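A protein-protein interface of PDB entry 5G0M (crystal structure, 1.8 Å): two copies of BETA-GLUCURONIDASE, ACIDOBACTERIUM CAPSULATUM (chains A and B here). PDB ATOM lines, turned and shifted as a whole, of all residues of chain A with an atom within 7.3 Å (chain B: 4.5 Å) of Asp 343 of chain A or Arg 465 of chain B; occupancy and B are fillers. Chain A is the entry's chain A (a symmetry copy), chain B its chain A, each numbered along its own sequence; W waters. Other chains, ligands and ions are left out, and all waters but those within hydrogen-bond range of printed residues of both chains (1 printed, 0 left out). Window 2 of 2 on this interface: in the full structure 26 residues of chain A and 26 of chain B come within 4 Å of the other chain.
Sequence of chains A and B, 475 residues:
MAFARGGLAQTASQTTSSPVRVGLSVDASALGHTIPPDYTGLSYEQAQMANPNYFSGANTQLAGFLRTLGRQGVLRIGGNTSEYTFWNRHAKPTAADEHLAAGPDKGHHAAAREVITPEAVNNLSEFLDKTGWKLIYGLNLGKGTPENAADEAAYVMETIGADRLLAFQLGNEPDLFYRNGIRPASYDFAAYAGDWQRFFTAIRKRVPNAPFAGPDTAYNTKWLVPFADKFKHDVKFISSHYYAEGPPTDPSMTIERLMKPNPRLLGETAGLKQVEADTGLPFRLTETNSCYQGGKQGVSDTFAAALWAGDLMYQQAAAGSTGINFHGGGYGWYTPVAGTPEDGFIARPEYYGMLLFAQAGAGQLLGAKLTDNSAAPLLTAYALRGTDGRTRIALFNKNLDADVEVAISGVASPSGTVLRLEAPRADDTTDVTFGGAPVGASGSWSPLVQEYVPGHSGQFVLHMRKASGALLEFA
O of Asp 343 of chain A is in hydrogen-bond range of OG1 of Thr 433 of chain B, at 2.7 Å. The backbone carbonyl oxygen (O) of Gly 436 of chain B lies within hydrogen-bond range of the side-chain amide nitrogen (NE2) of Gln 61 of chain A, 2.9 Å away. The side-chain carboxylate (OD1) of Asp 343 of chain A lies within salt-bridge range of the guanidinium group (NH1) of Arg 465 of chain B.
O of Arg 465 of chain B sits at hydrogen-bond distance from ND2 of Asn 397 of chain B, 2.8 Å away. N of Thr 433 of chain B sits at hydrogen-bond distance from O of Glu 422 of chain B (2.9 Å). The guanidinium group (NH1) of Arg 465 of chain B is in salt-bridge range of the side-chain carboxylate (OE1) of Glu 422 of chain B. The backbone carbonyl oxygen of Arg 465 of chain B sits at hydrogen-bond distance from the side-chain hydroxyl of Ser 468 of chain B (2.8 Å). The side-chain amide oxygen of Gln 61 of chain A sits at hydrogen-bond distance from the backbone NH of Phe 345 of chain A, 3.0 Å away. The side-chain hydroxyl (OG1) of Thr 340 of chain A is in hydrogen-bond range of the backbone NH (N) of Asp 343 of chain A, 2.9 Å away.
Among the printed residues, merely in contact across the chains: Asp 343 of chain A with Glu 422 of chain B, Asp 343 of chain A with Gly 436 of chain B and Gly 344 of chain A with Gly 436 of chain B.
Printed residues of chain B within 4 Å of Gln 61 of chain A: Gly 436 (2.9 Å). Asp 343 of chain A touches just these residues of chain B: Glu 422, Thr 433, Gly 436 and Arg 465. Of the printed residues of chain B, Gly 344 of chain A touches Gly 436. Of the printed residues of chain A, Glu 422 of chain B touches Asp 343 (3.6 Å). Printed residues of chain A within 4 Å of Thr 433 of chain B: Asp 343 (2.7 Å). Arg 465 of chain B touches one residue of chain A. The nearest residue of chain B that does not touch Asp 343 of chain A is Ala 437 of chain B (4.3 Å).
Of the 12 printed residues of chain B, 4 touch a printed residue of chain A. Along chain B the printed residues that touch a printed residue of chain A span positions 422 to 465. Of the 11 printed residues of chain A, 3 touch a printed residue of chain B. Printed residues of chain A that touch a printed residue of chain B: Gln 61, Asp 343 and Gly 344. Among the printed residues, 6 pairs touch across the chains.
No position is printed for both chains. Of the 6 pairs that touch across the chains among the printed residues, none has its exchanged pair printed and touching as well.
Water W1 lies within hydrogen-bond range of O of Glu 342 of chain A (2.8 Å) and N of Gly 436 of chain B (3.4 Å).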
ATOM      1  N   GLN A  61      30.799  16.873 -12.262  1.00  0.00           N
ATOM      2  CA  GLN A  61      31.624  16.485 -11.149  1.00  0.00           C
ATOM      3  C   GLN A  61      31.803  14.977 -11.097  1.00  0.00           C
ATOM      4  O   GLN A  61      32.924  14.509 -11.030  1.00  0.00           O
ATOM      5  CB  GLN A  61      31.053  16.987  -9.821  1.00  0.00           C
ATOM      6  CG  GLN A  61      30.983  18.518  -9.614  1.00  0.00           C
ATOM      7  CD  GLN A  61      30.648  18.888  -8.152  1.00  0.00           C
ATOM      8  OE1 GLN A  61      31.140  18.234  -7.197  1.00  0.00           O
ATOM      9  NE2 GLN A  61      29.828  19.912  -7.971  1.00  0.00           N
ATOM     10  N   HIS A  99      15.691  15.004  -6.442  1.00  0.00           N
ATOM     11  CA  HIS A  99      16.653  15.198  -5.349  1.00  0.00           C
ATOM     12  C   HIS A  99      17.093  13.873  -4.676  1.00  0.00           C
ATOM     13  O   HIS A  99      17.836  13.888  -3.703  1.00  0.00           O
ATOM     14  CB  HIS A  99      16.036  16.093  -4.276  1.00  0.00           C
ATOM     15  CG  HIS A  99      15.689  17.468  -4.742  1.00  0.00           C
ATOM     16  ND1 HIS A  99      16.531  18.545  -4.576  1.00  0.00           N
ATOM     17  CD2 HIS A  99      14.565  17.955  -5.320  1.00  0.00           C
ATOM     18  CE1 HIS A  99      15.953  19.631  -5.048  1.00  0.00           C
ATOM     19  NE2 HIS A  99      14.762  19.298  -5.515  1.00  0.00           N
ATOM     20  N   TYR A 331      26.102   8.400   0.350  1.00  0.00           N
ATOM     21  CA  TYR A 331      27.156   8.598   1.300  1.00  0.00           C
ATOM     22  C   TYR A 331      27.424   7.317   2.027  1.00  0.00           C
ATOM     23  O   TYR A 331      27.914   7.344   3.173  1.00  0.00           O
ATOM     24  CB  TYR A 331      26.820   9.723   2.297  1.00  0.00           C
ATOM     25  CG  TYR A 331      26.655  11.102   1.640  1.00  0.00           C
ATOM     26  CD1 TYR A 331      27.745  11.894   1.341  1.00  0.00           C
ATOM     27  CD2 TYR A 331      25.399  11.569   1.261  1.00  0.00           C
ATOM     28  CE1 TYR A 331      27.583  13.169   0.747  1.00  0.00           C
ATOM     29  CE2 TYR A 331      25.225  12.835   0.645  1.00  0.00           C
ATOM     30  CZ  TYR A 331      26.312  13.639   0.408  1.00  0.00           C
ATOM     31  OH  TYR A 331      26.110  14.871  -0.247  1.00  0.00           O
ATOM     32  N   GLY A 339      28.533  11.803  -2.463  1.00  0.00           N
ATOM     33  CA  GLY A 339      27.887  13.099  -2.761  1.00  0.00           C
ATOM     34  C   GLY A 339      26.558  13.173  -3.511  1.00  0.00           C
ATOM     35  O   GLY A 339      25.916  12.173  -3.726  1.00  0.00           O
ATOM     36  N   THR A 340      26.233  14.367  -4.017  1.00  0.00           N
ATOM     37  CA  THR A 340      24.972  14.631  -4.766  1.00  0.00           C
ATOM     38  C   THR A 340      25.192  15.704  -5.764  1.00  0.00           C
ATOM     39  O   THR A 340      26.105  16.513  -5.615  1.00  0.00           O
ATOM     40  CB  THR A 340      23.776  15.076  -3.855  1.00  0.00           C
ATOM     41  OG1 THR A 340      24.003  16.413  -3.352  1.00  0.00           O
ATOM     42  CG2 THR A 340      23.535  14.135  -2.651  1.00  0.00           C
ATOM     43  N   PRO A 341      24.335  15.787  -6.779  1.00  0.00           N
ATOM     44  CA  PRO A 341      24.507  16.941  -7.659  1.00  0.00           C
ATOM     45  C   PRO A 341      24.348  18.357  -6.994  1.00  0.00           C
ATOM     46  O   PRO A 341      25.057  19.276  -7.370  1.00  0.00           O
ATOM     47  CB  PRO A 341      23.508  16.687  -8.794  1.00  0.00           C
ATOM     48  CG  PRO A 341      23.041  15.275  -8.628  1.00  0.00           C
ATOM     49  CD  PRO A 341      23.255  14.877  -7.205  1.00  0.00           C
ATOM     50  N   GLU A 342      23.464  18.479  -6.008  1.00  0.00           N
ATOM     51  CA  GLU A 342      23.186  19.746  -5.272  1.00  0.00           C
ATOM     52  C   GLU A 342      24.364  20.116  -4.361  1.00  0.00           C
ATOM     53  O   GLU A 342      24.758  21.276  -4.263  1.00  0.00           O
ATOM     54  CB  GLU A 342      21.942  19.611  -4.373  1.00  0.00           C
ATOM     55  CG  GLU A 342      20.624  19.333  -5.074  1.00  0.00           C
ATOM     56  CD  GLU A 342      20.317  17.824  -5.385  1.00  0.00           C
ATOM     57  OE1 GLU A 342      21.073  16.873  -5.127  1.00  0.00           O
ATOM     58  OE2 GLU A 342      19.235  17.590  -5.945  1.00  0.00           O
ATOM     59  N   ASP A 343      24.934  19.115  -3.711  1.00  0.00           N
ATOM     60  CA  ASP A 343      25.994  19.381  -2.692  1.00  0.00           C
ATOM     61  C   ASP A 343      27.415  19.173  -3.181  1.00  0.00           C
ATOM     62  O   ASP A 343      28.377  19.569  -2.488  1.00  0.00           O
ATOM     63  CB  ASP A 343      25.733  18.538  -1.458  1.00  0.00           C
ATOM     64  CG  ASP A 343      24.374  18.838  -0.823  1.00  0.00           C
ATOM     65  OD1 ASP A 343      24.028  20.003  -0.608  1.00  0.00           O
ATOM     66  OD2 ASP A 343      23.652  17.898  -0.560  1.00  0.00           O
ATOM     67  N   GLY A 344      27.583  18.511  -4.334  1.00  0.00           N
ATOM     68  CA  GLY A 344      28.915  18.108  -4.787  1.00  0.00           C
ATOM     69  C   GLY A 344      29.412  16.733  -4.341  1.00  0.00           C
ATOM     70  O   GLY A 344      28.804  16.100  -3.527  1.00  0.00           O
ATOM     71  N   PHE A 345      30.514  16.302  -4.955  1.00  0.00           N
ATOM     72  CA  PHE A 345      31.026  14.975  -4.841  1.00  0.00           C
ATOM     73  C   PHE A 345      32.461  15.026  -4.328  1.00  0.00           C
ATOM     74  O   PHE A 345      33.169  15.989  -4.613  1.00  0.00           O
ATOM     75  CB  PHE A 345      30.988  14.209  -6.172  1.00  0.00           C
ATOM     76  CG  PHE A 345      29.598  13.879  -6.632  1.00  0.00           C
ATOM     77  CD1 PHE A 345      28.868  14.780  -7.341  1.00  0.00           C
ATOM     78  CD2 PHE A 345      29.007  12.656  -6.331  1.00  0.00           C
ATOM     79  CE1 PHE A 345      27.572  14.498  -7.764  1.00  0.00           C
ATOM     80  CE2 PHE A 345      27.722  12.367  -6.744  1.00  0.00           C
ATOM     81  CZ  PHE A 345      26.994  13.282  -7.477  1.00  0.00           C
ATOM     82  N   ILE A 346      32.861  13.995  -3.569  1.00  0.00           N
ATOM     83  CA  ILE A 346      34.259  13.856  -3.084  1.00  0.00           C
ATOM     84  C   ILE A 346      34.750  12.448  -3.158  1.00  0.00           C
ATOM     85  O   ILE A 346      33.929  11.499  -3.103  1.00  0.00           O
ATOM     86  CB  ILE A 346      34.403  14.258  -1.609  1.00  0.00           C
ATOM     87  CG1 ILE A 346      33.746  13.247  -0.709  1.00  0.00           C
ATOM     88  CG2 ILE A 346      33.768  15.622  -1.323  1.00  0.00           C
ATOM     89  CD1 ILE A 346      34.626  12.962   0.477  1.00  0.00           C
ATOM     90  N   ASN B 397      22.935  27.905  10.506  1.00  0.00           N
ATOM     91  CA  ASN B 397      21.851  27.196  11.113  1.00  0.00           C
ATOM     92  C   ASN B 397      22.435  26.070  11.940  1.00  0.00           C
ATOM     93  O   ASN B 397      22.563  24.946  11.459  1.00  0.00           O
ATOM     94  CB  ASN B 397      20.857  26.611  10.093  1.00  0.00           C
ATOM     95  CG  ASN B 397      19.632  26.017  10.789  1.00  0.00           C
ATOM     96  OD1 ASN B 397      19.400  26.309  11.980  1.00  0.00           O
ATOM     97  ND2 ASN B 397      18.876  25.129  10.085  1.00  0.00           N
ATOM     98  N   ASP B 403      15.112  22.512  10.341  1.00  0.00           N
ATOM     99  CA  ASP B 403      15.235  23.283   9.091  1.00  0.00           C
ATOM    100  C   ASP B 403      14.667  24.677   9.338  1.00  0.00           C
ATOM    101  O   ASP B 403      13.808  24.859  10.212  1.00  0.00           O
ATOM    102  CB  ASP B 403      14.426  22.617   7.959  1.00  0.00           C
ATOM    103  CG  ASP B 403      14.895  21.177   7.619  1.00  0.00           C
ATOM    104  OD1 ASP B 403      16.102  20.843   7.758  1.00  0.00           O
ATOM    105  OD2 ASP B 403      14.046  20.371   7.147  1.00  0.00           O
ATOM    106  N   GLU B 422      27.860  22.666   3.594  1.00  0.00           N
ATOM    107  CA  GLU B 422      27.102  21.404   3.763  1.00  0.00           C
ATOM    108  C   GLU B 422      27.951  20.170   4.097  1.00  0.00           C
ATOM    109  O   GLU B 422      29.076  19.985   3.655  1.00  0.00           O
ATOM    110  CB  GLU B 422      26.308  21.070   2.499  1.00  0.00           C
ATOM    111  CG  GLU B 422      25.289  22.087   1.988  1.00  0.00           C
ATOM    112  CD  GLU B 422      23.957  22.175   2.761  1.00  0.00           C
ATOM    113  OE1 GLU B 422      23.652  21.424   3.725  1.00  0.00           O
ATOM    114  OE2 GLU B 422      23.173  23.068   2.395  1.00  0.00           O
ATOM    115  N   THR B 433      31.371  20.222   1.888  1.00  0.00           N
ATOM    116  CA  THR B 433      31.517  21.065   0.723  1.00  0.00           C
ATOM    117  C   THR B 433      31.122  22.513   1.006  1.00  0.00           C
ATOM    118  O   THR B 433      30.345  22.808   1.901  1.00  0.00           O
ATOM    119  CB  THR B 433      30.713  20.503  -0.491  1.00  0.00           C
ATOM    120  OG1 THR B 433      29.343  20.461  -0.161  1.00  0.00           O
ATOM    121  CG2 THR B 433      31.221  19.121  -0.853  1.00  0.00           C
ATOM    122  N   GLY B 436      29.037  23.920  -3.270  1.00  0.00           N
ATOM    123  CA  GLY B 436      29.006  22.662  -4.021  1.00  0.00           C
ATOM    124  C   GLY B 436      30.302  22.010  -4.487  1.00  0.00           C
ATOM    125  O   GLY B 436      30.234  21.160  -5.398  1.00  0.00           O
ATOM    126  N   ALA B 437      31.441  22.308  -3.801  1.00  0.00           N
ATOM    127  CA  ALA B 437      32.761  21.784  -4.156  1.00  0.00           C
ATOM    128  C   ALA B 437      33.612  21.553  -2.892  1.00  0.00           C
ATOM    129  O   ALA B 437      33.510  22.328  -1.938  1.00  0.00           O
ATOM    130  CB  ALA B 437      33.517  22.737  -5.095  1.00  0.00           C
ATOM    131  N   HIS B 463      15.599  28.996   2.344  1.00  0.00           N
ATOM    132  CA  HIS B 463      15.546  27.729   3.101  1.00  0.00           C
ATOM    133  C   HIS B 463      16.981  27.302   3.427  1.00  0.00           C
ATOM    134  O   HIS B 463      17.902  27.534   2.647  1.00  0.00           O
ATOM    135  CB  HIS B 463      14.844  26.594   2.307  1.00  0.00           C
ATOM    136  CG  HIS B 463      14.607  25.320   3.090  1.00  0.00           C
ATOM    137  ND1 HIS B 463      15.383  24.184   2.947  1.00  0.00           N
ATOM    138  CD2 HIS B 463      13.654  24.999   3.999  1.00  0.00           C
ATOM    139  CE1 HIS B 463      14.932  23.234   3.746  1.00  0.00           C
ATOM    140  NE2 HIS B 463      13.886  23.705   4.401  1.00  0.00           N
ATOM    141  N   MET B 464      17.140  26.693   4.591  1.00  0.00           N
ATOM    142  CA  MET B 464      18.392  26.043   5.056  1.00  0.00           C
ATOM    143  C   MET B 464      18.028  24.776   5.829  1.00  0.00           C
ATOM    144  O   MET B 464      17.260  24.822   6.758  1.00  0.00           O
ATOM    145  CB  MET B 464      19.168  26.970   6.048  1.00  0.00           C
ATOM    146  CG  MET B 464      19.497  28.352   5.555  1.00  0.00           C
ATOM    147  SD  MET B 464      20.467  29.354   6.718  1.00  0.00           S
ATOM    148  CE  MET B 464      22.052  28.479   6.629  1.00  0.00           C
ATOM    149  N   ARG B 465      18.693  23.682   5.532  1.00  0.00           N
ATOM    150  CA  ARG B 465      18.565  22.456   6.295  1.00  0.00           C
ATOM    151  C   ARG B 465      19.104  22.655   7.687  1.00  0.00           C
ATOM    152  O   ARG B 465      19.861  23.574   7.930  1.00  0.00           O
ATOM    153  CB  ARG B 465      19.401  21.329   5.685  1.00  0.00           C
ATOM    154  CG  ARG B 465      19.088  20.934   4.267  1.00  0.00           C
ATOM    155  CD  ARG B 465      20.227  20.026   3.795  1.00  0.00           C
ATOM    156  NE  ARG B 465      20.081  19.595   2.404  1.00  0.00           N
ATOM    157  CZ  ARG B 465      21.092  19.303   1.561  1.00  0.00           C
ATOM    158  NH1 ARG B 465      22.380  19.397   1.931  1.00  0.00           N
ATOM    159  NH2 ARG B 465      20.808  18.917   0.303  1.00  0.00           N
ATOM    160  N   LYS B 466      18.689  21.781   8.587  1.00  0.00           N
ATOM    161  CA  LYS B 466      19.311  21.631   9.874  1.00  0.00           C
ATOM    162  C   LYS B 466      20.823  21.453   9.677  1.00  0.00           C
ATOM    163  O   LYS B 466      21.293  20.776   8.694  1.00  0.00           O
ATOM    164  CB  LYS B 466      18.709  20.392  10.623  1.00  0.00           C
ATOM    165  CG  LYS B 466      18.871  19.076   9.841  1.00  0.00           C
ATOM    166  CD  LYS B 466      18.195  17.874  10.499  1.00  0.00           C
ATOM    167  CE  LYS B 466      18.337  16.687   9.545  1.00  0.00           C
ATOM    168  NZ  LYS B 466      18.038  15.423  10.267  1.00  0.00           N
ATOM    169  N   ALA B 467      21.597  22.050  10.576  1.00  0.00           N
ATOM    170  CA  ALA B 467      23.073  21.830  10.598  1.00  0.00           C
ATOM    171  C   ALA B 467      23.697  22.106   9.224  1.00  0.00           C
ATOM    172  O   ALA B 467      24.295  21.240   8.549  1.00  0.00           O
ATOM    173  CB  ALA B 467      23.439  20.476  11.143  1.00  0.00           C
ATOM    174  N   SER B 468      23.510  23.365   8.803  1.00  0.00           N
ATOM    175  CA  SER B 468      24.084  23.897   7.582  1.00  0.00           C
ATOM    176  C   SER B 468      24.404  25.385   7.727  1.00  0.00           C
ATOM    177  O   SER B 468      23.987  26.071   8.674  1.00  0.00           O
ATOM    178  CB  SER B 468      23.132  23.705   6.398  1.00  0.00           C
ATOM    179  OG  SER B 468      22.088  24.614   6.530  1.00  0.00           O
HETATM  180  O   HOH W   1      25.773  23.165  -2.466  1.00  0.00           O
